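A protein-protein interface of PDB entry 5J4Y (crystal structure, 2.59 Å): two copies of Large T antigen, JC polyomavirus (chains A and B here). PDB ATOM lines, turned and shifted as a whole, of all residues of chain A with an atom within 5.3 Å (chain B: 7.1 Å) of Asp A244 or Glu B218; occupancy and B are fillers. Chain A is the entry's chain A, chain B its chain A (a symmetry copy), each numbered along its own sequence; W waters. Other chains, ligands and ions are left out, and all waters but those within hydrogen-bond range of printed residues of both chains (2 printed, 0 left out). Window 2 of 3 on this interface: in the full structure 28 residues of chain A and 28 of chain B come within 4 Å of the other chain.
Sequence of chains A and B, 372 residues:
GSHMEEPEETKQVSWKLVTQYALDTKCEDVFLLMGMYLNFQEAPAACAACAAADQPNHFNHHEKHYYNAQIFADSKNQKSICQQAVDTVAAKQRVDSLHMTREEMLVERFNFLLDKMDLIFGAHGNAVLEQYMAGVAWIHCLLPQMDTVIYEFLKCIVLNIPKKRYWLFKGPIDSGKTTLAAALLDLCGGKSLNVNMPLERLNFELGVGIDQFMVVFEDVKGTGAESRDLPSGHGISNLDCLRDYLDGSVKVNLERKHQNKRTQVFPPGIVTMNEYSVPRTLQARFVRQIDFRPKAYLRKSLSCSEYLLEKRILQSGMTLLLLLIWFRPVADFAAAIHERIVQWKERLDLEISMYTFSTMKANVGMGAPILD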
ATOM      1  N   CYS A 241     -23.408  12.830  19.746  1.00  0.00           N
ATOM      2  CA  CYS A 241     -23.106  13.152  18.348  1.00  0.00           C
ATOM      3  C   CYS A 241     -22.103  14.304  18.212  1.00  0.00           C
ATOM      4  O   CYS A 241     -21.437  14.413  17.184  1.00  0.00           O
ATOM      5  CB  CYS A 241     -24.391  13.441  17.582  1.00  0.00           C
ATOM      6  SG  CYS A 241     -25.623  12.118  17.692  1.00  0.00           S
ATOM      7  N   LEU A 242     -21.982  15.145  19.254  1.00  0.00           N
ATOM      8  CA  LEU A 242     -21.073  16.297  19.269  1.00  0.00           C
ATOM      9  C   LEU A 242     -19.702  15.951  19.885  1.00  0.00           C
ATOM     10  O   LEU A 242     -19.059  16.800  20.508  1.00  0.00           O
ATOM     11  CB  LEU A 242     -21.745  17.518  19.946  1.00  0.00           C
ATOM     12  CG  LEU A 242     -23.106  17.934  19.358  1.00  0.00           C
ATOM     13  CD1 LEU A 242     -23.896  18.766  20.329  1.00  0.00           C
ATOM     14  CD2 LEU A 242     -22.964  18.618  18.004  1.00  0.00           C
ATOM     15  N   ARG A 243     -19.249  14.700  19.660  1.00  0.00           N
ATOM     16  CA  ARG A 243     -17.990  14.145  20.154  1.00  0.00           C
ATOM     17  C   ARG A 243     -16.785  15.030  19.818  1.00  0.00           C
ATOM     18  O   ARG A 243     -15.945  15.260  20.689  1.00  0.00           O
ATOM     19  CB  ARG A 243     -17.791  12.714  19.600  1.00  0.00           C
ATOM     20  CG  ARG A 243     -16.703  11.909  20.320  1.00  0.00           C
ATOM     21  CD  ARG A 243     -16.259  10.708  19.507  1.00  0.00           C
ATOM     22  NE  ARG A 243     -14.800  10.569  19.474  1.00  0.00           N
ATOM     23  CZ  ARG A 243     -14.141   9.693  18.717  1.00  0.00           C
ATOM     24  NH1 ARG A 243     -14.800   8.867  17.912  1.00  0.00           N
ATOM     25  NH2 ARG A 243     -12.814   9.644  18.752  1.00  0.00           N
ATOM     26  N   ASP A 244     -16.717  15.520  18.560  1.00  0.00           N
ATOM     27  CA  ASP A 244     -15.645  16.362  18.004  1.00  0.00           C
ATOM     28  C   ASP A 244     -15.501  17.691  18.737  1.00  0.00           C
ATOM     29  O   ASP A 244     -14.387  18.192  18.928  1.00  0.00           O
ATOM     30  CB  ASP A 244     -15.888  16.654  16.506  1.00  0.00           C
ATOM     31  CG  ASP A 244     -16.938  15.801  15.801  1.00  0.00           C
ATOM     32  OD1 ASP A 244     -18.131  15.839  16.231  1.00  0.00           O
ATOM     33  OD2 ASP A 244     -16.584  15.139  14.785  1.00  0.00           O
ATOM     34  N   TYR A 245     -16.647  18.267  19.112  1.00  0.00           N
ATOM     35  CA  TYR A 245     -16.787  19.541  19.805  1.00  0.00           C
ATOM     36  C   TYR A 245     -16.299  19.428  21.249  1.00  0.00           C
ATOM     37  O   TYR A 245     -15.454  20.226  21.682  1.00  0.00           O
ATOM     38  CB  TYR A 245     -18.261  19.984  19.749  1.00  0.00           C
ATOM     39  CG  TYR A 245     -18.806  20.275  18.360  1.00  0.00           C
ATOM     40  CD1 TYR A 245     -19.047  19.243  17.447  1.00  0.00           C
ATOM     41  CD2 TYR A 245     -19.171  21.565  17.993  1.00  0.00           C
ATOM     42  CE1 TYR A 245     -19.598  19.502  16.191  1.00  0.00           C
ATOM     43  CE2 TYR A 245     -19.714  21.836  16.740  1.00  0.00           C
ATOM     44  CZ  TYR A 245     -19.938  20.802  15.846  1.00  0.00           C
ATOM     45  OH  TYR A 245     -20.496  21.104  14.629  1.00  0.00           O
ATOM     46  N   LEU A 246     -16.801  18.408  21.977  1.00  0.00           N
ATOM     47  CA  LEU A 246     -16.449  18.139  23.371  1.00  0.00           C
ATOM     48  C   LEU A 246     -15.014  17.649  23.544  1.00  0.00           C
ATOM     49  O   LEU A 246     -14.420  17.903  24.596  1.00  0.00           O
ATOM     50  CB  LEU A 246     -17.411  17.111  24.002  1.00  0.00           C
ATOM     51  CG  LEU A 246     -18.909  17.464  24.165  1.00  0.00           C
ATOM     52  CD1 LEU A 246     -19.612  16.417  25.016  1.00  0.00           C
ATOM     53  CD2 LEU A 246     -19.109  18.830  24.791  1.00  0.00           C
ATOM     54  N   ASP A 247     -14.465  16.905  22.548  1.00  0.00           N
ATOM     55  CA  ASP A 247     -13.103  16.374  22.664  1.00  0.00           C
ATOM     56  C   ASP A 247     -12.032  17.412  22.322  1.00  0.00           C
ATOM     57  O   ASP A 247     -11.022  17.467  23.014  1.00  0.00           O
ATOM     58  CB  ASP A 247     -12.913  15.060  21.896  1.00  0.00           C
ATOM     59  CG  ASP A 247     -13.366  13.813  22.652  1.00  0.00           C
ATOM     60  OD1 ASP A 247     -13.613  13.911  23.879  1.00  0.00           O
ATOM     61  OD2 ASP A 247     -13.459  12.732  22.020  1.00  0.00           O
ATOM     62  N   GLY A 248     -12.271  18.247  21.317  1.00  0.00           N
ATOM     63  CA  GLY A 248     -11.356  19.326  20.945  1.00  0.00           C
ATOM     64  C   GLY A 248      -9.947  18.911  20.566  1.00  0.00           C
ATOM     65  O   GLY A 248      -8.970  19.490  21.056  1.00  0.00           O
ATOM     66  N   SER A 249      -9.845  17.889  19.698  1.00  0.00           N
ATOM     67  CA  SER A 249      -8.599  17.356  19.140  1.00  0.00           C
ATOM     68  C   SER A 249      -8.502  17.921  17.710  1.00  0.00           C
ATOM     69  O   SER A 249      -7.419  18.264  17.227  1.00  0.00           O
ATOM     70  CB  SER A 249      -8.650  15.828  19.076  1.00  0.00           C
ATOM     71  OG  SER A 249      -9.164  15.232  20.256  1.00  0.00           O
ATOM     72  N   VAL A 250      -9.667  18.008  17.046  1.00  0.00           N
ATOM     73  CA  VAL A 250      -9.845  18.522  15.690  1.00  0.00           C
ATOM     74  C   VAL A 250     -10.673  19.814  15.747  1.00  0.00           C
ATOM     75  O   VAL A 250     -11.476  19.997  16.667  1.00  0.00           O
ATOM     76  CB  VAL A 250     -10.471  17.465  14.727  1.00  0.00           C
ATOM     77  CG1 VAL A 250      -9.663  16.181  14.735  1.00  0.00           C
ATOM     78  CG2 VAL A 250     -11.939  17.170  15.052  1.00  0.00           C
ATOM     79  N   VAL A 252     -13.627  22.397  14.286  1.00  0.00           N
ATOM     80  CA  VAL A 252     -14.999  22.181  13.815  1.00  0.00           C
ATOM     81  C   VAL A 252     -15.537  23.409  13.059  1.00  0.00           C
ATOM     82  O   VAL A 252     -15.066  24.522  13.298  1.00  0.00           O
ATOM     83  CB  VAL A 252     -15.942  21.707  14.946  1.00  0.00           C
ATOM     84  CG1 VAL A 252     -15.786  20.213  15.202  1.00  0.00           C
ATOM     85  CG2 VAL A 252     -15.718  22.498  16.232  1.00  0.00           C
ATOM     86  N   LYS B 177      -7.815   6.199  13.975  1.00  0.00           N
ATOM     87  CA  LYS B 177      -8.442   6.568  12.693  1.00  0.00           C
ATOM     88  C   LYS B 177      -8.732   8.087  12.555  1.00  0.00           C
ATOM     89  O   LYS B 177      -8.449   8.680  11.513  1.00  0.00           O
ATOM     90  CB  LYS B 177      -9.699   5.711  12.414  1.00  0.00           C
ATOM     91  CG  LYS B 177     -10.979   6.128  13.128  1.00  0.00           C
ATOM     92  CD  LYS B 177     -12.214   5.472  12.502  1.00  0.00           C
ATOM     93  CE  LYS B 177     -13.511   5.901  13.150  1.00  0.00           C
ATOM     94  NZ  LYS B 177     -13.592   5.477  14.557  1.00  0.00           N
ATOM     95  N   THR B 178      -9.260   8.702  13.616  1.00  0.00           N
ATOM     96  CA  THR B 178      -9.610  10.112  13.656  1.00  0.00           C
ATOM     97  C   THR B 178      -8.343  10.942  13.638  1.00  0.00           C
ATOM     98  O   THR B 178      -8.186  11.785  12.764  1.00  0.00           O
ATOM     99  CB  THR B 178     -10.568  10.358  14.829  1.00  0.00           C
ATOM    100  OG1 THR B 178     -11.779   9.650  14.549  1.00  0.00           O
ATOM    101  CG2 THR B 178     -10.870  11.835  15.058  1.00  0.00           C
ATOM    102  N   THR B 179      -7.413  10.642  14.550  1.00  0.00           N
ATOM    103  CA  THR B 179      -6.118  11.301  14.689  1.00  0.00           C
ATOM    104  C   THR B 179      -5.355  11.364  13.367  1.00  0.00           C
ATOM    105  O   THR B 179      -4.921  12.448  12.986  1.00  0.00           O
ATOM    106  CB  THR B 179      -5.299  10.639  15.815  1.00  0.00           C
ATOM    107  OG1 THR B 179      -6.115  10.564  16.981  1.00  0.00           O
ATOM    108  CG2 THR B 179      -4.056  11.419  16.160  1.00  0.00           C
ATOM    109  N   ALA B 181      -6.569  10.715  10.224  1.00  0.00           N
ATOM    110  CA  ALA B 181      -7.388  11.401   9.206  1.00  0.00           C
ATOM    111  C   ALA B 181      -7.245  12.905   9.371  1.00  0.00           C
ATOM    112  O   ALA B 181      -7.098  13.612   8.385  1.00  0.00           O
ATOM    113  CB  ALA B 181      -8.845  10.995   9.335  1.00  0.00           C
ATOM    114  N   ALA B 182      -7.216  13.374  10.627  1.00  0.00           N
ATOM    115  CA  ALA B 182      -7.057  14.775  10.994  1.00  0.00           C
ATOM    116  C   ALA B 182      -5.667  15.274  10.585  1.00  0.00           C
ATOM    117  O   ALA B 182      -5.542  16.353   9.992  1.00  0.00           O
ATOM    118  CB  ALA B 182      -7.260  14.932  12.493  1.00  0.00           C
ATOM    119  N   LEU B 185      -5.436  15.437   6.840  1.00  0.00           N
ATOM    120  CA  LEU B 185      -6.292  16.565   6.449  1.00  0.00           C
ATOM    121  C   LEU B 185      -5.528  17.883   6.672  1.00  0.00           C
ATOM    122  O   LEU B 185      -5.574  18.782   5.838  1.00  0.00           O
ATOM    123  CB  LEU B 185      -7.605  16.543   7.252  1.00  0.00           C
ATOM    124  CG  LEU B 185      -8.615  17.663   6.987  1.00  0.00           C
ATOM    125  CD1 LEU B 185      -9.050  17.707   5.490  1.00  0.00           C
ATOM    126  CD2 LEU B 185      -9.833  17.512   7.891  1.00  0.00           C
ATOM    127  N   SER B 192     -13.253  18.993   6.726  1.00  0.00           N
ATOM    128  CA  SER B 192     -13.952  17.815   7.230  1.00  0.00           C
ATOM    129  C   SER B 192     -15.428  18.115   7.037  1.00  0.00           C
ATOM    130  O   SER B 192     -15.838  19.279   7.100  1.00  0.00           O
ATOM    131  CB  SER B 192     -13.629  17.540   8.696  1.00  0.00           C
ATOM    132  OG  SER B 192     -13.528  18.742   9.440  1.00  0.00           O
ATOM    133  N   LEU B 193     -16.200  17.075   6.711  1.00  0.00           N
ATOM    134  CA  LEU B 193     -17.619  17.165   6.415  1.00  0.00           C
ATOM    135  C   LEU B 193     -18.419  16.195   7.265  1.00  0.00           C
ATOM    136  O   LEU B 193     -17.971  15.068   7.518  1.00  0.00           O
ATOM    137  CB  LEU B 193     -17.876  16.858   4.925  1.00  0.00           C
ATOM    138  CG  LEU B 193     -17.028  17.563   3.839  1.00  0.00           C
ATOM    139  CD1 LEU B 193     -17.299  16.960   2.486  1.00  0.00           C
ATOM    140  CD2 LEU B 193     -17.318  19.053   3.778  1.00  0.00           C
ATOM    141  N   ASN B 194     -19.626  16.634   7.669  1.00  0.00           N
ATOM    142  CA  ASN B 194     -20.593  15.849   8.436  1.00  0.00           C
ATOM    143  C   ASN B 194     -21.815  15.479   7.568  1.00  0.00           C
ATOM    144  O   ASN B 194     -22.739  16.284   7.410  1.00  0.00           O
ATOM    145  CB  ASN B 194     -21.013  16.607   9.698  1.00  0.00           C
ATOM    146  CG  ASN B 194     -22.147  15.989  10.490  1.00  0.00           C
ATOM    147  OD1 ASN B 194     -22.218  14.768  10.700  1.00  0.00           O
ATOM    148  ND2 ASN B 194     -23.037  16.842  10.990  1.00  0.00           N
ATOM    149  N   VAL B 195     -21.812  14.258   7.011  1.00  0.00           N
ATOM    150  CA  VAL B 195     -22.921  13.760   6.183  1.00  0.00           C
ATOM    151  C   VAL B 195     -23.965  12.960   7.014  1.00  0.00           C
ATOM    152  O   VAL B 195     -24.756  12.231   6.420  1.00  0.00           O
ATOM    153  CB  VAL B 195     -22.484  12.979   4.893  1.00  0.00           C
ATOM    154  CG1 VAL B 195     -21.858  13.905   3.859  1.00  0.00           C
ATOM    155  CG2 VAL B 195     -21.568  11.794   5.205  1.00  0.00           C
ATOM    156  N   ASN B 196     -23.991  13.113   8.356  1.00  0.00           N
ATOM    157  CA  ASN B 196     -24.960  12.404   9.216  1.00  0.00           C
ATOM    158  C   ASN B 196     -26.359  13.051   9.222  1.00  0.00           C
ATOM    159  O   ASN B 196     -27.345  12.391   9.560  1.00  0.00           O
ATOM    160  CB  ASN B 196     -24.424  12.206  10.626  1.00  0.00           C
ATOM    161  CG  ASN B 196     -23.358  11.146  10.706  1.00  0.00           C
ATOM    162  OD1 ASN B 196     -22.286  11.352  11.287  1.00  0.00           O
ATOM    163  ND2 ASN B 196     -23.627   9.989  10.113  1.00  0.00           N
ATOM    164  N   VAL B 215     -11.129  16.272   1.226  1.00  0.00           N
ATOM    165  CA  VAL B 215     -12.172  16.259   2.256  1.00  0.00           C
ATOM    166  C   VAL B 215     -12.095  14.984   3.110  1.00  0.00           C
ATOM    167  O   VAL B 215     -11.588  13.957   2.652  1.00  0.00           O
ATOM    168  CB  VAL B 215     -13.622  16.510   1.722  1.00  0.00           C
ATOM    169  CG1 VAL B 215     -13.771  17.878   1.040  1.00  0.00           C
ATOM    170  CG2 VAL B 215     -14.106  15.376   0.817  1.00  0.00           C
ATOM    171  N   VAL B 216     -12.607  15.059   4.353  1.00  0.00           N
ATOM    172  CA  VAL B 216     -12.708  13.921   5.284  1.00  0.00           C
ATOM    173  C   VAL B 216     -14.153  13.871   5.680  1.00  0.00           C
ATOM    174  O   VAL B 216     -14.649  14.861   6.194  1.00  0.00           O
ATOM    175  CB  VAL B 216     -11.796  13.988   6.557  1.00  0.00           C
ATOM    176  CG1 VAL B 216     -11.987  12.751   7.439  1.00  0.00           C
ATOM    177  CG2 VAL B 216     -10.321  14.150   6.193  1.00  0.00           C
ATOM    178  N   PHE B 217     -14.837  12.749   5.420  1.00  0.00           N
ATOM    179  CA  PHE B 217     -16.228  12.539   5.825  1.00  0.00           C
ATOM    180  C   PHE B 217     -16.052  11.912   7.175  1.00  0.00           C
ATOM    181  O   PHE B 217     -15.811  10.705   7.264  1.00  0.00           O
ATOM    182  CB  PHE B 217     -16.943  11.593   4.850  1.00  0.00           C
ATOM    183  CG  PHE B 217     -17.251  12.219   3.518  1.00  0.00           C
ATOM    184  CD1 PHE B 217     -18.391  12.989   3.342  1.00  0.00           C
ATOM    185  CD2 PHE B 217     -16.418  12.013   2.428  1.00  0.00           C
ATOM    186  CE1 PHE B 217     -18.691  13.545   2.098  1.00  0.00           C
ATOM    187  CE2 PHE B 217     -16.720  12.567   1.185  1.00  0.00           C
ATOM    188  CZ  PHE B 217     -17.862  13.319   1.024  1.00  0.00           C
ATOM    189  N   GLU B 218     -16.013  12.758   8.217  1.00  0.00           N
ATOM    190  CA  GLU B 218     -15.668  12.327   9.570  1.00  0.00           C
ATOM    191  C   GLU B 218     -16.834  11.692  10.306  1.00  0.00           C
ATOM    192  O   GLU B 218     -17.920  12.278  10.395  1.00  0.00           O
ATOM    193  CB  GLU B 218     -15.014  13.484  10.368  1.00  0.00           C
ATOM    194  CG  GLU B 218     -14.775  13.268  11.864  1.00  0.00           C
ATOM    195  CD  GLU B 218     -13.934  12.076  12.290  1.00  0.00           C
ATOM    196  OE1 GLU B 218     -14.378  11.335  13.197  1.00  0.00           O
ATOM    197  OE2 GLU B 218     -12.819  11.897  11.745  1.00  0.00           O
ATOM    198  N   ASP B 219     -16.574  10.482  10.848  1.00  0.00           N
ATOM    199  CA  ASP B 219     -17.460   9.667  11.681  1.00  0.00           C
ATOM    200  C   ASP B 219     -18.840   9.370  11.054  1.00  0.00           C
ATOM    201  O   ASP B 219     -19.892   9.670  11.632  1.00  0.00           O
ATOM    202  CB  ASP B 219     -17.602  10.283  13.076  1.00  0.00           C
ATOM    203  CG  ASP B 219     -17.592   9.253  14.183  1.00  0.00           C
ATOM    204  OD1 ASP B 219     -16.658   8.396  14.194  1.00  0.00           O
ATOM    205  OD2 ASP B 219     -18.468   9.337  15.080  1.00  0.00           O
ATOM    206  N   VAL B 220     -18.814   8.735   9.895  1.00  0.00           N
ATOM    207  CA  VAL B 220     -19.998   8.362   9.138  1.00  0.00           C
ATOM    208  C   VAL B 220     -20.753   7.233   9.892  1.00  0.00           C
ATOM    209  O   VAL B 220     -20.139   6.252  10.315  1.00  0.00           O
ATOM    210  CB  VAL B 220     -19.561   7.995   7.701  1.00  0.00           C
ATOM    211  CG1 VAL B 220     -20.705   7.395   6.899  1.00  0.00           C
ATOM    212  CG2 VAL B 220     -18.973   9.210   6.979  1.00  0.00           C
ATOM    213  N   LYS B 221     -22.069   7.416  10.115  1.00  0.00           N
ATOM    214  CA  LYS B 221     -22.891   6.459  10.865  1.00  0.00           C
ATOM    215  C   LYS B 221     -23.849   5.680   9.971  1.00  0.00           C
ATOM    216  O   LYS B 221     -24.378   6.230   9.016  1.00  0.00           O
ATOM    217  CB  LYS B 221     -23.686   7.152  11.992  1.00  0.00           C
ATOM    218  CG  LYS B 221     -22.850   7.760  13.104  1.00  0.00           C
ATOM    219  CD  LYS B 221     -23.727   8.389  14.178  1.00  0.00           C
ATOM    220  CE  LYS B 221     -23.884   9.887  14.036  1.00  0.00           C
ATOM    221  NZ  LYS B 221     -25.004  10.417  14.868  1.00  0.00           N
ATOM    222  N   ILE B 270     -10.749  11.013   2.560  1.00  0.00           N
ATOM    223  CA  ILE B 270     -11.027   9.903   3.480  1.00  0.00           C
ATOM    224  C   ILE B 270     -12.499   9.921   3.965  1.00  0.00           C
ATOM    225  O   ILE B 270     -13.162  10.961   3.997  1.00  0.00           O
ATOM    226  CB  ILE B 270     -10.029   9.920   4.712  1.00  0.00           C
ATOM    227  CG1 ILE B 270      -8.562  10.035   4.272  1.00  0.00           C
ATOM    228  CG2 ILE B 270     -10.180   8.694   5.607  1.00  0.00           C
ATOM    229  CD1 ILE B 270      -7.601  10.862   5.204  1.00  0.00           C
ATOM    230  N   VAL B 271     -12.973   8.741   4.334  1.00  0.00           N
ATOM    231  CA  VAL B 271     -14.209   8.448   5.037  1.00  0.00           C
ATOM    232  C   VAL B 271     -13.768   7.711   6.364  1.00  0.00           C
ATOM    233  O   VAL B 271     -13.000   6.730   6.310  1.00  0.00           O
ATOM    234  CB  VAL B 271     -15.165   7.577   4.180  1.00  0.00           C
ATOM    235  CG1 VAL B 271     -16.300   7.008   5.023  1.00  0.00           C
ATOM    236  CG2 VAL B 271     -15.716   8.361   2.986  1.00  0.00           C
ATOM    237  N   THR B 272     -14.206   8.209   7.541  1.00  0.00           N
ATOM    238  CA  THR B 272     -13.954   7.502   8.811  1.00  0.00           C
ATOM    239  C   THR B 272     -15.305   7.014   9.351  1.00  0.00           C
ATOM    240  O   THR B 272     -16.325   7.677   9.126  1.00  0.00           O
ATOM    241  CB  THR B 272     -13.070   8.270   9.825  1.00  0.00           C
ATOM    242  OG1 THR B 272     -13.770   9.388  10.333  1.00  0.00           O
ATOM    243  CG2 THR B 272     -11.752   8.731   9.238  1.00  0.00           C
ATOM    244  N   MET B 273     -15.326   5.831   9.985  1.00  0.00           N
ATOM    245  CA  MET B 273     -16.538   5.217  10.536  1.00  0.00           C
ATOM    246  C   MET B 273     -16.236   4.117  11.555  1.00  0.00           C
ATOM    247  O   MET B 273     -15.130   3.580  11.566  1.00  0.00           O
ATOM    248  CB  MET B 273     -17.422   4.650   9.406  1.00  0.00           C
ATOM    249  CG  MET B 273     -16.758   3.572   8.533  1.00  0.00           C
ATOM    250  SD  MET B 273     -17.890   2.897   7.270  1.00  0.00           S
ATOM    251  CE  MET B 273     -18.576   1.624   8.161  1.00  0.00           C
HETATM  252  O   HOH W   1     -15.601  10.874  16.155  1.00  0.00           O
HETATM  253  O   HOH W   2     -12.330   7.456  16.451  1.00  0.00           O
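The side-chain sulfur (SG) of Cys A241 sits at hydrogen-bond distance from the side-chain amino group (NZ) of Lys B221 (3.4 Å).
OE2 of Glu B218 is in hydrogen-bond range of OG1 of Thr B272.
N of Glu B218 is in hydrogen-bond range of O of Leu B193.
The side-chain carboxylate of Glu B218 sits at hydrogen-bond distance from the side-chain hydroxyl of Thr B178 (3.4 Å).
The side-chain amide nitrogen (ND2) of Asn B196 lies close to the backbone NH (N) of Lys B221 (3.0 Å).
CG of Glu B218 touches OD2 of Asp A244, at 3.9 Å.
Val A250 touches Ala B182.
Of the printed residues of chain B, Cys A241 touches Lys B221 (3.4 Å).
Of chain B, only Glu B218 (3.9 Å) comes within 4 Å of Asp A244.
Asp A247 touches none of the printed residues of chain B.
Of the printed residues of chain B, Val A250 touches Ala B182 (3.5 Å).
Printed residues of chain A within 4 Å of Ala B182: Val A250 (3.5 Å).
Val B195 touches none of the printed residues of chain A.
Glu B218 touches just one residue of chain A: Asp A244.
Of the 22 printed residues of chain B, 3 touch a printed residue of chain A.
Hydrophobic or aromatic side chains of chain B that line the printed part of chain A: Ala B182.
Along chain A the printed residues that touch a printed residue of chain B span positions 241 to 250.
Among the printed residues, no Asp or Glu carboxylate lies within 4 Å of a Lys or Arg side-chain nitrogen of the other chain.
No position is printed for both chains.
Water W1 lies within hydrogen-bond range of the guanidinium group (NH1) of Arg A243 (2.8 Å), the side-chain carboxylate (OE1) of Glu B218 (3.2 Å) and the side-chain carboxylate (OD1) of Asp B219 (3.3 Å).
Water W2 lies within hydrogen-bond range of OG1 of Thr B178 (3.0 Å), NZ of Lys B177 (3.0 Å) and NH1 of Arg A243 (3.2 Å).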
